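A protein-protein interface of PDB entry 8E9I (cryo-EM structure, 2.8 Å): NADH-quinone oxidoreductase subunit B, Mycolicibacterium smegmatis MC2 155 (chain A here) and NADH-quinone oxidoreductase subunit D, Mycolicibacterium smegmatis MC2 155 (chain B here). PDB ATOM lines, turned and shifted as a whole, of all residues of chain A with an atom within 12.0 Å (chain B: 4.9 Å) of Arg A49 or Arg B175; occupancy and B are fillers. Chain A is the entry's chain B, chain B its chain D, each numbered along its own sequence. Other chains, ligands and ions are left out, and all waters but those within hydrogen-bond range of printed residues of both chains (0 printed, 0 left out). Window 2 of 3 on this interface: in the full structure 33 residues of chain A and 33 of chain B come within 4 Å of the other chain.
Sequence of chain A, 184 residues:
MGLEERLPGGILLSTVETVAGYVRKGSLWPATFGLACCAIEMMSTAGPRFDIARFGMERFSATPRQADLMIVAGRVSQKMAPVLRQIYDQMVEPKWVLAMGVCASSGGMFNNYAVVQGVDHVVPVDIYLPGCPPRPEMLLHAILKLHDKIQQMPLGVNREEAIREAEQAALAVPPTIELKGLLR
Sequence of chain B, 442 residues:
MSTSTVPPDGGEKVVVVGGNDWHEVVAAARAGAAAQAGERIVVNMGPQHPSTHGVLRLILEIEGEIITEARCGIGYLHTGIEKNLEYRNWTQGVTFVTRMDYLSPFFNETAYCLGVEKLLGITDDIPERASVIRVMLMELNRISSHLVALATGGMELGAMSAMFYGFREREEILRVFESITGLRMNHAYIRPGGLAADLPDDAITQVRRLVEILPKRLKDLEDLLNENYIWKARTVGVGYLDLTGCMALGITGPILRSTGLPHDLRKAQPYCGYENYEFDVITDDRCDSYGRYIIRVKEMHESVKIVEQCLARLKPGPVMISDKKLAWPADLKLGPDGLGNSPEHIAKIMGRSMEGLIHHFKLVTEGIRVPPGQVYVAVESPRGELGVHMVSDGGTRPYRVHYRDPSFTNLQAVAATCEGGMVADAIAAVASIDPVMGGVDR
The guanidinium group (NH1) of Arg A135 is in salt-bridge range of the side-chain carboxylate (OE2) of Glu B178 (3.1 Å).
NH1 of Arg B184 sits close to NH1 of Arg A49.
NE of Arg A49 sits close to NH2 of Arg B175, 3.3 Å away.
The side-chain carboxylate (OE1) of Glu A41 is in salt-bridge range of the guanidinium group (NE) of Arg B184, at 3.0 Å.
The side-chain carboxylate (OE1) of Glu B171 lies within salt-bridge range of the guanidinium group (NH1) of Arg A49.
The backbone carbonyl oxygen (O) of Glu A41 sits at hydrogen-bond distance from the side-chain hydroxyl (OG1) of Thr A45.
The side-chain hydroxyl (OG) of Ser B179 is in hydrogen-bond range of the backbone carbonyl oxygen (O) of Arg B175.
The backbone carbonyl oxygen (O) of Ile A40 sits at hydrogen-bond distance from the side-chain hydroxyl (OG) of Ser A44, at 2.9 Å.
The side-chain carboxylate of Glu B171 is in salt-bridge range of the guanidinium group of Arg B184.
The backbone NH (N) of Arg A135 lies close to the side-chain sulfur (SD) of Met A138 (3.8 Å).
Among the printed residues, merely in contact across the chains: Ser A44 with Glu B171, Ser A44 with Arg B184, Phe A50 with Glu B171, Arg A135 with Arg B184 and Pro A136 with Arg B184.
Of the printed residues of chain B, Glu A41 touches Arg B184.
Of the printed residues of chain B, Ser A44 touches Glu B171 and Arg B184.
Gly A47 touches none of the printed residues of chain B.
Arg A49 touches three residues of chain B.
Of the printed residues of chain B, Arg A135 touches Glu B178 and Arg B184.
Of the printed residues of chain B, Pro A136 touches Arg B184.
Of chain A, only Ser A44 (3.5 Å), Arg A49 (2.8 Å) and Phe A50 (3.9 Å) come within 4 Å of Glu B171.
No residue of chain A comes within 4 Å of Glu B172.
Arg B175 touches just one residue of chain A: Arg A49.
No residue of chain A comes within 4 Å of Val B176.
No residue of chain A comes within 4 Å of Phe B177.
Printed residues of chain B that touch a printed residue of chain A: Glu B171, Arg B175, Glu B178 and Arg B184.
Among the printed residues, Asp or Glu carboxylates within 4 Å of a Lys or Arg side-chain nitrogen of the other chain: Glu A41 with Arg B184, Arg A49 with Glu B171 and Arg A135 with Glu B178.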
ATOM      1  N   ILE A  40     -14.409   3.670  23.906  1.00  0.00           N
ATOM      2  CA  ILE A  40     -14.681   3.700  22.478  1.00  0.00           C
ATOM      3  C   ILE A  40     -13.393   3.909  21.704  1.00  0.00           C
ATOM      4  O   ILE A  40     -13.157   3.251  20.686  1.00  0.00           O
ATOM      5  CB  ILE A  40     -15.718   4.787  22.149  1.00  0.00           C
ATOM      6  CG1 ILE A  40     -16.980   4.605  22.994  1.00  0.00           C
ATOM      7  CG2 ILE A  40     -16.013   4.809  20.672  1.00  0.00           C
ATOM      8  CD1 ILE A  40     -17.626   3.253  22.878  1.00  0.00           C
ATOM      9  N   GLU A  41     -12.531   4.819  22.163  1.00  0.00           N
ATOM     10  CA  GLU A  41     -11.282   5.002  21.430  1.00  0.00           C
ATOM     11  C   GLU A  41     -10.385   3.778  21.538  1.00  0.00           C
ATOM     12  O   GLU A  41      -9.613   3.499  20.622  1.00  0.00           O
ATOM     13  CB  GLU A  41     -10.540   6.244  21.906  1.00  0.00           C
ATOM     14  CG  GLU A  41     -11.078   7.522  21.300  1.00  0.00           C
ATOM     15  CD  GLU A  41     -10.918   7.577  19.788  1.00  0.00           C
ATOM     16  OE1 GLU A  41      -9.919   7.038  19.279  1.00  0.00           O
ATOM     17  OE2 GLU A  41     -11.798   8.141  19.109  1.00  0.00           O
ATOM     18  N   MET A  42     -10.478   3.033  22.633  1.00  0.00           N
ATOM     19  CA  MET A  42      -9.716   1.797  22.750  1.00  0.00           C
ATOM     20  C   MET A  42     -10.211   0.766  21.743  1.00  0.00           C
ATOM     21  O   MET A  42      -9.417   0.082  21.084  1.00  0.00           O
ATOM     22  CB  MET A  42      -9.817   1.277  24.182  1.00  0.00           C
ATOM     23  CG  MET A  42      -9.025   0.024  24.464  1.00  0.00           C
ATOM     24  SD  MET A  42      -9.189  -0.489  26.180  1.00  0.00           S
ATOM     25  CE  MET A  42     -10.871  -1.085  26.202  1.00  0.00           C
ATOM     26  N   MET A  43     -11.532   0.648  21.597  1.00  0.00           N
ATOM     27  CA  MET A  43     -12.062  -0.232  20.559  1.00  0.00           C
ATOM     28  C   MET A  43     -11.616   0.229  19.179  1.00  0.00           C
ATOM     29  O   MET A  43     -11.261  -0.588  18.325  1.00  0.00           O
ATOM     30  CB  MET A  43     -13.588  -0.316  20.616  1.00  0.00           C
ATOM     31  CG  MET A  43     -14.122  -0.992  21.850  1.00  0.00           C
ATOM     32  SD  MET A  43     -15.920  -1.157  21.870  1.00  0.00           S
ATOM     33  CE  MET A  43     -16.428   0.518  22.203  1.00  0.00           C
ATOM     34  N   SER A  44     -11.621   1.539  18.947  1.00  0.00           N
ATOM     35  CA  SER A  44     -11.124   2.069  17.684  1.00  0.00           C
ATOM     36  C   SER A  44      -9.662   1.709  17.459  1.00  0.00           C
ATOM     37  O   SER A  44      -9.272   1.407  16.327  1.00  0.00           O
ATOM     38  CB  SER A  44     -11.304   3.585  17.656  1.00  0.00           C
ATOM     39  OG  SER A  44     -12.634   3.945  17.971  1.00  0.00           O
ATOM     40  N   THR A  45      -8.848   1.739  18.510  1.00  0.00           N
ATOM     41  CA  THR A  45      -7.464   1.295  18.414  1.00  0.00           C
ATOM     42  C   THR A  45      -7.376  -0.166  18.017  1.00  0.00           C
ATOM     43  O   THR A  45      -6.526  -0.532  17.202  1.00  0.00           O
ATOM     44  CB  THR A  45      -6.745   1.494  19.747  1.00  0.00           C
ATOM     45  OG1 THR A  45      -6.963   2.826  20.221  1.00  0.00           O
ATOM     46  CG2 THR A  45      -5.256   1.246  19.590  1.00  0.00           C
ATOM     47  N   ALA A  46      -8.230  -1.011  18.591  1.00  0.00           N
ATOM     48  CA  ALA A  46      -8.266  -2.406  18.169  1.00  0.00           C
ATOM     49  C   ALA A  46      -8.816  -2.542  16.755  1.00  0.00           C
ATOM     50  O   ALA A  46      -8.581  -3.556  16.089  1.00  0.00           O
ATOM     51  CB  ALA A  46      -9.103  -3.226  19.146  1.00  0.00           C
ATOM     52  N   GLY A  47      -9.549  -1.539  16.282  1.00  0.00           N
ATOM     53  CA  GLY A  47     -10.165  -1.580  14.977  1.00  0.00           C
ATOM     54  C   GLY A  47      -9.158  -1.575  13.848  1.00  0.00           C
ATOM     55  O   GLY A  47      -7.993  -1.229  14.033  1.00  0.00           O
ATOM     56  N   PRO A  48      -9.605  -1.943  12.642  1.00  0.00           N
ATOM     57  CA  PRO A  48      -8.667  -2.152  11.529  1.00  0.00           C
ATOM     58  C   PRO A  48      -7.858  -0.934  11.133  1.00  0.00           C
ATOM     59  O   PRO A  48      -6.721  -1.110  10.684  1.00  0.00           O
ATOM     60  CB  PRO A  48      -9.584  -2.588  10.383  1.00  0.00           C
ATOM     61  CG  PRO A  48     -10.897  -2.003  10.723  1.00  0.00           C
ATOM     62  CD  PRO A  48     -10.999  -2.102  12.207  1.00  0.00           C
ATOM     63  N   ARG A  49      -8.381   0.287  11.261  1.00  0.00           N
ATOM     64  CA  ARG A  49      -7.588   1.441  10.847  1.00  0.00           C
ATOM     65  C   ARG A  49      -6.230   1.419  11.527  1.00  0.00           C
ATOM     66  O   ARG A  49      -5.218   1.805  10.934  1.00  0.00           O
ATOM     67  CB  ARG A  49      -8.315   2.744  11.162  1.00  0.00           C
ATOM     68  CG  ARG A  49      -7.509   3.970  10.767  1.00  0.00           C
ATOM     69  CD  ARG A  49      -8.190   5.263  11.151  1.00  0.00           C
ATOM     70  NE  ARG A  49      -7.292   6.395  10.973  1.00  0.00           N
ATOM     71  CZ  ARG A  49      -7.517   7.615  11.438  1.00  0.00           C
ATOM     72  NH1 ARG A  49      -8.621   7.909  12.101  1.00  0.00           N
ATOM     73  NH2 ARG A  49      -6.608   8.563  11.232  1.00  0.00           N
ATOM     74  N   PHE A  50      -6.198   0.983  12.771  1.00  0.00           N
ATOM     75  CA  PHE A  50      -4.990   0.612  13.481  1.00  0.00           C
ATOM     76  C   PHE A  50      -5.024  -0.896  13.679  1.00  0.00           C
ATOM     77  O   PHE A  50      -5.882  -1.593  13.143  1.00  0.00           O
ATOM     78  CB  PHE A  50      -4.914   1.366  14.804  1.00  0.00           C
ATOM     79  CG  PHE A  50      -5.277   2.808  14.678  1.00  0.00           C
ATOM     80  CD1 PHE A  50      -4.329   3.750  14.336  1.00  0.00           C
ATOM     81  CD2 PHE A  50      -6.584   3.218  14.856  1.00  0.00           C
ATOM     82  CE1 PHE A  50      -4.675   5.073  14.206  1.00  0.00           C
ATOM     83  CE2 PHE A  50      -6.928   4.535  14.721  1.00  0.00           C
ATOM     84  CZ  PHE A  50      -5.978   5.462  14.399  1.00  0.00           C
ATOM     85  N   ASP A  51      -4.059  -1.422  14.421  1.00  0.00           N
ATOM     86  CA  ASP A  51      -4.136  -2.838  14.765  1.00  0.00           C
ATOM     87  C   ASP A  51      -3.353  -3.035  16.063  1.00  0.00           C
ATOM     88  O   ASP A  51      -2.147  -3.276  16.038  1.00  0.00           O
ATOM     89  CB  ASP A  51      -3.602  -3.715  13.653  1.00  0.00           C
ATOM     90  N   ILE A  52      -4.062  -2.964  17.185  1.00  0.00           N
ATOM     91  CA  ILE A  52      -3.444  -3.280  18.455  1.00  0.00           C
ATOM     92  C   ILE A  52      -2.944  -4.711  18.459  1.00  0.00           C
ATOM     93  O   ILE A  52      -1.933  -5.012  19.099  1.00  0.00           O
ATOM     94  CB  ILE A  52      -4.452  -3.022  19.593  1.00  0.00           C
ATOM     95  CG1 ILE A  52      -3.742  -2.953  20.943  1.00  0.00           C
ATOM     96  CG2 ILE A  52      -5.513  -4.098  19.615  1.00  0.00           C
ATOM     97  CD1 ILE A  52      -4.575  -2.303  22.023  1.00  0.00           C
ATOM     98  N   ALA A  53      -3.606  -5.592  17.707  1.00  0.00           N
ATOM     99  CA  ALA A  53      -3.147  -6.968  17.582  1.00  0.00           C
ATOM    100  C   ALA A  53      -1.711  -7.039  17.094  1.00  0.00           C
ATOM    101  O   ALA A  53      -0.996  -7.988  17.427  1.00  0.00           O
ATOM    102  CB  ALA A  53      -4.058  -7.738  16.631  1.00  0.00           C
ATOM    103  N   ARG A  54      -1.270  -6.057  16.305  1.00  0.00           N
ATOM    104  CA  ARG A  54       0.117  -6.056  15.855  1.00  0.00           C
ATOM    105  C   ARG A  54       1.070  -6.223  17.024  1.00  0.00           C
ATOM    106  O   ARG A  54       2.055  -6.961  16.922  1.00  0.00           O
ATOM    107  CB  ARG A  54       0.437  -4.765  15.105  1.00  0.00           C
ATOM    108  CG  ARG A  54      -0.174  -4.671  13.727  1.00  0.00           C
ATOM    109  CD  ARG A  54       0.120  -3.328  13.086  1.00  0.00           C
ATOM    110  NE  ARG A  54      -0.487  -2.227  13.827  1.00  0.00           N
ATOM    111  CZ  ARG A  54       0.081  -1.051  14.045  1.00  0.00           C
ATOM    112  NH1 ARG A  54       1.306  -0.781  13.630  1.00  0.00           N
ATOM    113  NH2 ARG A  54      -0.603  -0.112  14.692  1.00  0.00           N
ATOM    114  N   PHE A  55       0.779  -5.581  18.145  1.00  0.00           N
ATOM    115  CA  PHE A  55       1.644  -5.621  19.311  1.00  0.00           C
ATOM    116  C   PHE A  55       1.342  -6.801  20.218  1.00  0.00           C
ATOM    117  O   PHE A  55       1.624  -6.730  21.416  1.00  0.00           O
ATOM    118  CB  PHE A  55       1.509  -4.315  20.087  1.00  0.00           C
ATOM    119  CG  PHE A  55       1.574  -3.107  19.213  1.00  0.00           C
ATOM    120  CD1 PHE A  55       2.783  -2.520  18.916  1.00  0.00           C
ATOM    121  CD2 PHE A  55       0.426  -2.573  18.664  1.00  0.00           C
ATOM    122  CE1 PHE A  55       2.846  -1.423  18.099  1.00  0.00           C
ATOM    123  CE2 PHE A  55       0.484  -1.475  17.849  1.00  0.00           C
ATOM    124  CZ  PHE A  55       1.693  -0.898  17.566  1.00  0.00           C
ATOM    125  N   PRO A 133     -10.885  12.119  24.144  1.00  0.00           N
ATOM    126  CA  PRO A 133     -10.095  10.927  24.449  1.00  0.00           C
ATOM    127  C   PRO A 133      -8.748  10.950  23.762  1.00  0.00           C
ATOM    128  O   PRO A 133      -8.623  11.609  22.738  1.00  0.00           O
ATOM    129  CB  PRO A 133     -10.951   9.804  23.892  1.00  0.00           C
ATOM    130  CG  PRO A 133     -11.613  10.422  22.723  1.00  0.00           C
ATOM    131  CD  PRO A 133     -11.853  11.858  23.068  1.00  0.00           C
ATOM    132  N   PRO A 134      -7.759  10.244  24.299  1.00  0.00           N
ATOM    133  CA  PRO A 134      -6.514  10.067  23.550  1.00  0.00           C
ATOM    134  C   PRO A 134      -6.789   9.333  22.251  1.00  0.00           C
ATOM    135  O   PRO A 134      -7.441   8.288  22.240  1.00  0.00           O
ATOM    136  CB  PRO A 134      -5.638   9.242  24.496  1.00  0.00           C
ATOM    137  CG  PRO A 134      -6.554   8.651  25.478  1.00  0.00           C
ATOM    138  CD  PRO A 134      -7.712   9.573  25.606  1.00  0.00           C
ATOM    139  N   ARG A 135      -6.297   9.883  21.149  1.00  0.00           N
ATOM    140  CA  ARG A 135      -6.511   9.216  19.886  1.00  0.00           C
ATOM    141  C   ARG A 135      -5.746   7.897  19.878  1.00  0.00           C
ATOM    142  O   ARG A 135      -4.786   7.722  20.628  1.00  0.00           O
ATOM    143  CB  ARG A 135      -6.074  10.091  18.718  1.00  0.00           C
ATOM    144  CG  ARG A 135      -4.598  10.392  18.678  1.00  0.00           C
ATOM    145  CD  ARG A 135      -4.268  11.219  17.460  1.00  0.00           C
ATOM    146  NE  ARG A 135      -4.618  10.508  16.236  1.00  0.00           N
ATOM    147  CZ  ARG A 135      -5.173  11.060  15.167  1.00  0.00           C
ATOM    148  NH1 ARG A 135      -5.450  12.353  15.115  1.00  0.00           N
ATOM    149  NH2 ARG A 135      -5.450  10.297  14.115  1.00  0.00           N
ATOM    150  N   PRO A 136      -6.158   6.954  19.035  1.00  0.00           N
ATOM    151  CA  PRO A 136      -5.556   5.615  19.093  1.00  0.00           C
ATOM    152  C   PRO A 136      -4.051   5.622  18.918  1.00  0.00           C
ATOM    153  O   PRO A 136      -3.363   4.784  19.509  1.00  0.00           O
ATOM    154  CB  PRO A 136      -6.270   4.883  17.953  1.00  0.00           C
ATOM    155  CG  PRO A 136      -7.569   5.610  17.821  1.00  0.00           C
ATOM    156  CD  PRO A 136      -7.185   7.032  17.988  1.00  0.00           C
ATOM    157  N   GLU A 137      -3.511   6.549  18.128  1.00  0.00           N
ATOM    158  CA  GLU A 137      -2.062   6.646  18.017  1.00  0.00           C
ATOM    159  C   GLU A 137      -1.429   6.977  19.361  1.00  0.00           C
ATOM    160  O   GLU A 137      -0.372   6.437  19.699  1.00  0.00           O
ATOM    161  CB  GLU A 137      -1.684   7.693  16.971  1.00  0.00           C
ATOM    162  N   MET A 138      -2.062   7.845  20.150  1.00  0.00           N
ATOM    163  CA  MET A 138      -1.539   8.135  21.480  1.00  0.00           C
ATOM    164  C   MET A 138      -1.635   6.921  22.392  1.00  0.00           C
ATOM    165  O   MET A 138      -0.736   6.686  23.207  1.00  0.00           O
ATOM    166  CB  MET A 138      -2.280   9.316  22.101  1.00  0.00           C
ATOM    167  CG  MET A 138      -1.985  10.638  21.440  1.00  0.00           C
ATOM    168  SD  MET A 138      -3.192  11.918  21.812  1.00  0.00           S
ATOM    169  CE  MET A 138      -3.251  11.819  23.594  1.00  0.00           C
ATOM    170  N   LEU A 139      -2.712   6.143  22.281  1.00  0.00           N
ATOM    171  CA  LEU A 139      -2.805   4.927  23.078  1.00  0.00           C
ATOM    172  C   LEU A 139      -1.689   3.960  22.720  1.00  0.00           C
ATOM    173  O   LEU A 139      -1.079   3.352  23.605  1.00  0.00           O
ATOM    174  CB  LEU A 139      -4.164   4.264  22.882  1.00  0.00           C
ATOM    175  CG  LEU A 139      -4.277   2.884  23.529  1.00  0.00           C
ATOM    176  CD1 LEU A 139      -3.922   2.959  24.998  1.00  0.00           C
ATOM    177  CD2 LEU A 139      -5.666   2.316  23.342  1.00  0.00           C
ATOM    178  N   LEU A 140      -1.411   3.799  21.428  1.00  0.00           N
ATOM    179  CA  LEU A 140      -0.321   2.921  21.029  1.00  0.00           C
ATOM    180  C   LEU A 140       1.013   3.454  21.526  1.00  0.00           C
ATOM    181  O   LEU A 140       1.888   2.681  21.927  1.00  0.00           O
ATOM    182  CB  LEU A 140      -0.307   2.755  19.512  1.00  0.00           C
ATOM    183  CG  LEU A 140      -1.570   2.140  18.914  1.00  0.00           C
ATOM    184  CD1 LEU A 140      -1.473   2.091  17.405  1.00  0.00           C
ATOM    185  CD2 LEU A 140      -1.820   0.758  19.476  1.00  0.00           C
ATOM    186  N   GLU B 171     -14.523   4.626  11.259  1.00  0.00           N
ATOM    187  CA  GLU B 171     -13.311   5.404  11.061  1.00  0.00           C
ATOM    188  C   GLU B 171     -13.426   6.260   9.818  1.00  0.00           C
ATOM    189  O   GLU B 171     -12.905   7.384   9.780  1.00  0.00           O
ATOM    190  CB  GLU B 171     -12.105   4.473  10.956  1.00  0.00           C
ATOM    191  CG  GLU B 171     -11.650   3.912  12.289  1.00  0.00           C
ATOM    192  CD  GLU B 171     -10.990   4.955  13.166  1.00  0.00           C
ATOM    193  OE1 GLU B 171     -10.650   6.037  12.642  1.00  0.00           O
ATOM    194  OE2 GLU B 171     -10.820   4.699  14.378  1.00  0.00           O
ATOM    195  N   GLU B 172     -14.104   5.747   8.789  1.00  0.00           N
ATOM    196  CA  GLU B 172     -14.379   6.571   7.619  1.00  0.00           C
ATOM    197  C   GLU B 172     -15.052   7.882   8.016  1.00  0.00           C
ATOM    198  O   GLU B 172     -14.728   8.940   7.470  1.00  0.00           O
ATOM    199  CB  GLU B 172     -15.250   5.803   6.627  1.00  0.00           C
ATOM    200  N   ILE B 173     -15.975   7.834   8.976  1.00  0.00           N
ATOM    201  CA  ILE B 173     -16.683   9.043   9.394  1.00  0.00           C
ATOM    202  C   ILE B 173     -15.850   9.843  10.389  1.00  0.00           C
ATOM    203  O   ILE B 173     -15.913  11.079  10.426  1.00  0.00           O
ATOM    204  CB  ILE B 173     -18.051   8.678   9.991  1.00  0.00           C
ATOM    205  CG1 ILE B 173     -18.822   7.764   9.048  1.00  0.00           C
ATOM    206  CG2 ILE B 173     -18.848   9.928  10.254  1.00  0.00           C
ATOM    207  CD1 ILE B 173     -20.066   7.195   9.662  1.00  0.00           C
ATOM    208  N   LEU B 174     -15.088   9.157  11.236  1.00  0.00           N
ATOM    209  CA  LEU B 174     -14.300   9.861  12.236  1.00  0.00           C
ATOM    210  C   LEU B 174     -13.186  10.667  11.596  1.00  0.00           C
ATOM    211  O   LEU B 174     -12.749  11.668  12.165  1.00  0.00           O
ATOM    212  CB  LEU B 174     -13.719   8.889  13.261  1.00  0.00           C
ATOM    213  CG  LEU B 174     -14.646   8.283  14.315  1.00  0.00           C
ATOM    214  CD1 LEU B 174     -13.809   7.732  15.447  1.00  0.00           C
ATOM    215  CD2 LEU B 174     -15.655   9.278  14.855  1.00  0.00           C
ATOM    216  N   ARG B 175     -12.707  10.261  10.422  1.00  0.00           N
ATOM    217  CA  ARG B 175     -11.758  11.120   9.719  1.00  0.00           C
ATOM    218  C   ARG B 175     -12.398  12.445   9.329  1.00  0.00           C
ATOM    219  O   ARG B 175     -11.778  13.505   9.475  1.00  0.00           O
ATOM    220  CB  ARG B 175     -11.203  10.410   8.491  1.00  0.00           C
ATOM    221  CG  ARG B 175     -10.226   9.313   8.834  1.00  0.00           C
ATOM    222  CD  ARG B 175      -9.265   9.058   7.698  1.00  0.00           C
ATOM    223  NE  ARG B 175      -8.500   7.839   7.918  1.00  0.00           N
ATOM    224  CZ  ARG B 175      -8.953   6.619   7.670  1.00  0.00           C
ATOM    225  NH1 ARG B 175     -10.168   6.416   7.190  1.00  0.00           N
ATOM    226  NH2 ARG B 175      -8.165   5.575   7.911  1.00  0.00           N
ATOM    227  N   VAL B 176     -13.640  12.409   8.846  1.00  0.00           N
ATOM    228  CA  VAL B 176     -14.354  13.645   8.547  1.00  0.00           C
ATOM    229  C   VAL B 176     -14.549  14.467   9.810  1.00  0.00           C
ATOM    230  O   VAL B 176     -14.392  15.692   9.802  1.00  0.00           O
ATOM    231  CB  VAL B 176     -15.698  13.335   7.868  1.00  0.00           C
ATOM    232  CG1 VAL B 176     -16.563  14.571   7.845  1.00  0.00           C
ATOM    233  CG2 VAL B 176     -15.454  12.829   6.461  1.00  0.00           C
ATOM    234  N   PHE B 177     -14.921  13.815  10.907  1.00  0.00           N
ATOM    235  CA  PHE B 177     -15.082  14.548  12.157  1.00  0.00           C
ATOM    236  C   PHE B 177     -13.773  15.200  12.577  1.00  0.00           C
ATOM    237  O   PHE B 177     -13.760  16.353  13.017  1.00  0.00           O
ATOM    238  CB  PHE B 177     -15.582  13.620  13.261  1.00  0.00           C
ATOM    239  CG  PHE B 177     -16.994  13.152  13.079  1.00  0.00           C
ATOM    240  CD1 PHE B 177     -17.860  13.799  12.222  1.00  0.00           C
ATOM    241  CD2 PHE B 177     -17.456  12.059  13.785  1.00  0.00           C
ATOM    242  CE1 PHE B 177     -19.152  13.363  12.070  1.00  0.00           C
ATOM    243  CE2 PHE B 177     -18.749  11.619  13.634  1.00  0.00           C
ATOM    244  CZ  PHE B 177     -19.599  12.274  12.775  1.00  0.00           C
ATOM    245  N   GLU B 178     -12.662  14.476  12.454  1.00  0.00           N
ATOM    246  CA  GLU B 178     -11.370  15.032  12.829  1.00  0.00           C
ATOM    247  C   GLU B 178     -11.028  16.232  11.965  1.00  0.00           C
ATOM    248  O   GLU B 178     -10.541  17.250  12.470  1.00  0.00           O
ATOM    249  CB  GLU B 178     -10.287  13.960  12.714  1.00  0.00           C
ATOM    250  CG  GLU B 178      -8.925  14.383  13.241  1.00  0.00           C
ATOM    251  CD  GLU B 178      -7.856  13.332  13.009  1.00  0.00           C
ATOM    252  OE1 GLU B 178      -8.150  12.130  13.158  1.00  0.00           O
ATOM    253  OE2 GLU B 178      -6.713  13.707  12.673  1.00  0.00           O
ATOM    254  N   SER B 179     -11.273  16.135  10.658  1.00  0.00           N
ATOM    255  CA  SER B 179     -10.979  17.263   9.783  1.00  0.00           C
ATOM    256  C   SER B 179     -11.839  18.467  10.132  1.00  0.00           C
ATOM    257  O   SER B 179     -11.333  19.590  10.226  1.00  0.00           O
ATOM    258  CB  SER B 179     -11.191  16.870   8.327  1.00  0.00           C
ATOM    259  OG  SER B 179     -12.500  16.382   8.129  1.00  0.00           O
ATOM    260  N   ARG B 184     -11.728  13.543  17.492  1.00  0.00           N
ATOM    261  CA  ARG B 184     -12.359  12.314  17.042  1.00  0.00           C
ATOM    262  C   ARG B 184     -13.665  12.046  17.764  1.00  0.00           C
ATOM    263  O   ARG B 184     -14.604  11.519  17.161  1.00  0.00           O
ATOM    264  CB  ARG B 184     -11.406  11.137  17.244  1.00  0.00           C
ATOM    265  CG  ARG B 184     -10.238  11.165  16.291  1.00  0.00           C
ATOM    266  CD  ARG B 184      -9.166  10.184  16.690  1.00  0.00           C
ATOM    267  NE  ARG B 184      -9.719   8.851  16.883  1.00  0.00           N
ATOM    268  CZ  ARG B 184     -10.066   8.041  15.894  1.00  0.00           C
ATOM    269  NH1 ARG B 184      -9.964   8.411  14.629  1.00  0.00           N
ATOM    270  NH2 ARG B 184     -10.536   6.831  16.183  1.00  0.00           N
ATOM    271  N   GLN B 206     -14.663  15.488   1.396  1.00  0.00           N
ATOM    272  CA  GLN B 206     -14.610  14.321   2.268  1.00  0.00           C
ATOM    273  C   GLN B 206     -16.003  13.763   2.517  1.00  0.00           C
ATOM    274  O   GLN B 206     -16.206  12.545   2.494  1.00  0.00           O
ATOM    275  CB  GLN B 206     -13.947  14.688   3.594  1.00  0.00           C
ATOM    276  CG  GLN B 206     -12.536  15.214   3.459  1.00  0.00           C
ATOM    277  CD  GLN B 206     -11.773  15.179   4.764  1.00  0.00           C
ATOM    278  OE1 GLN B 206     -12.027  14.338   5.624  1.00  0.00           O
ATOM    279  NE2 GLN B 206     -10.838  16.106   4.925  1.00  0.00           N
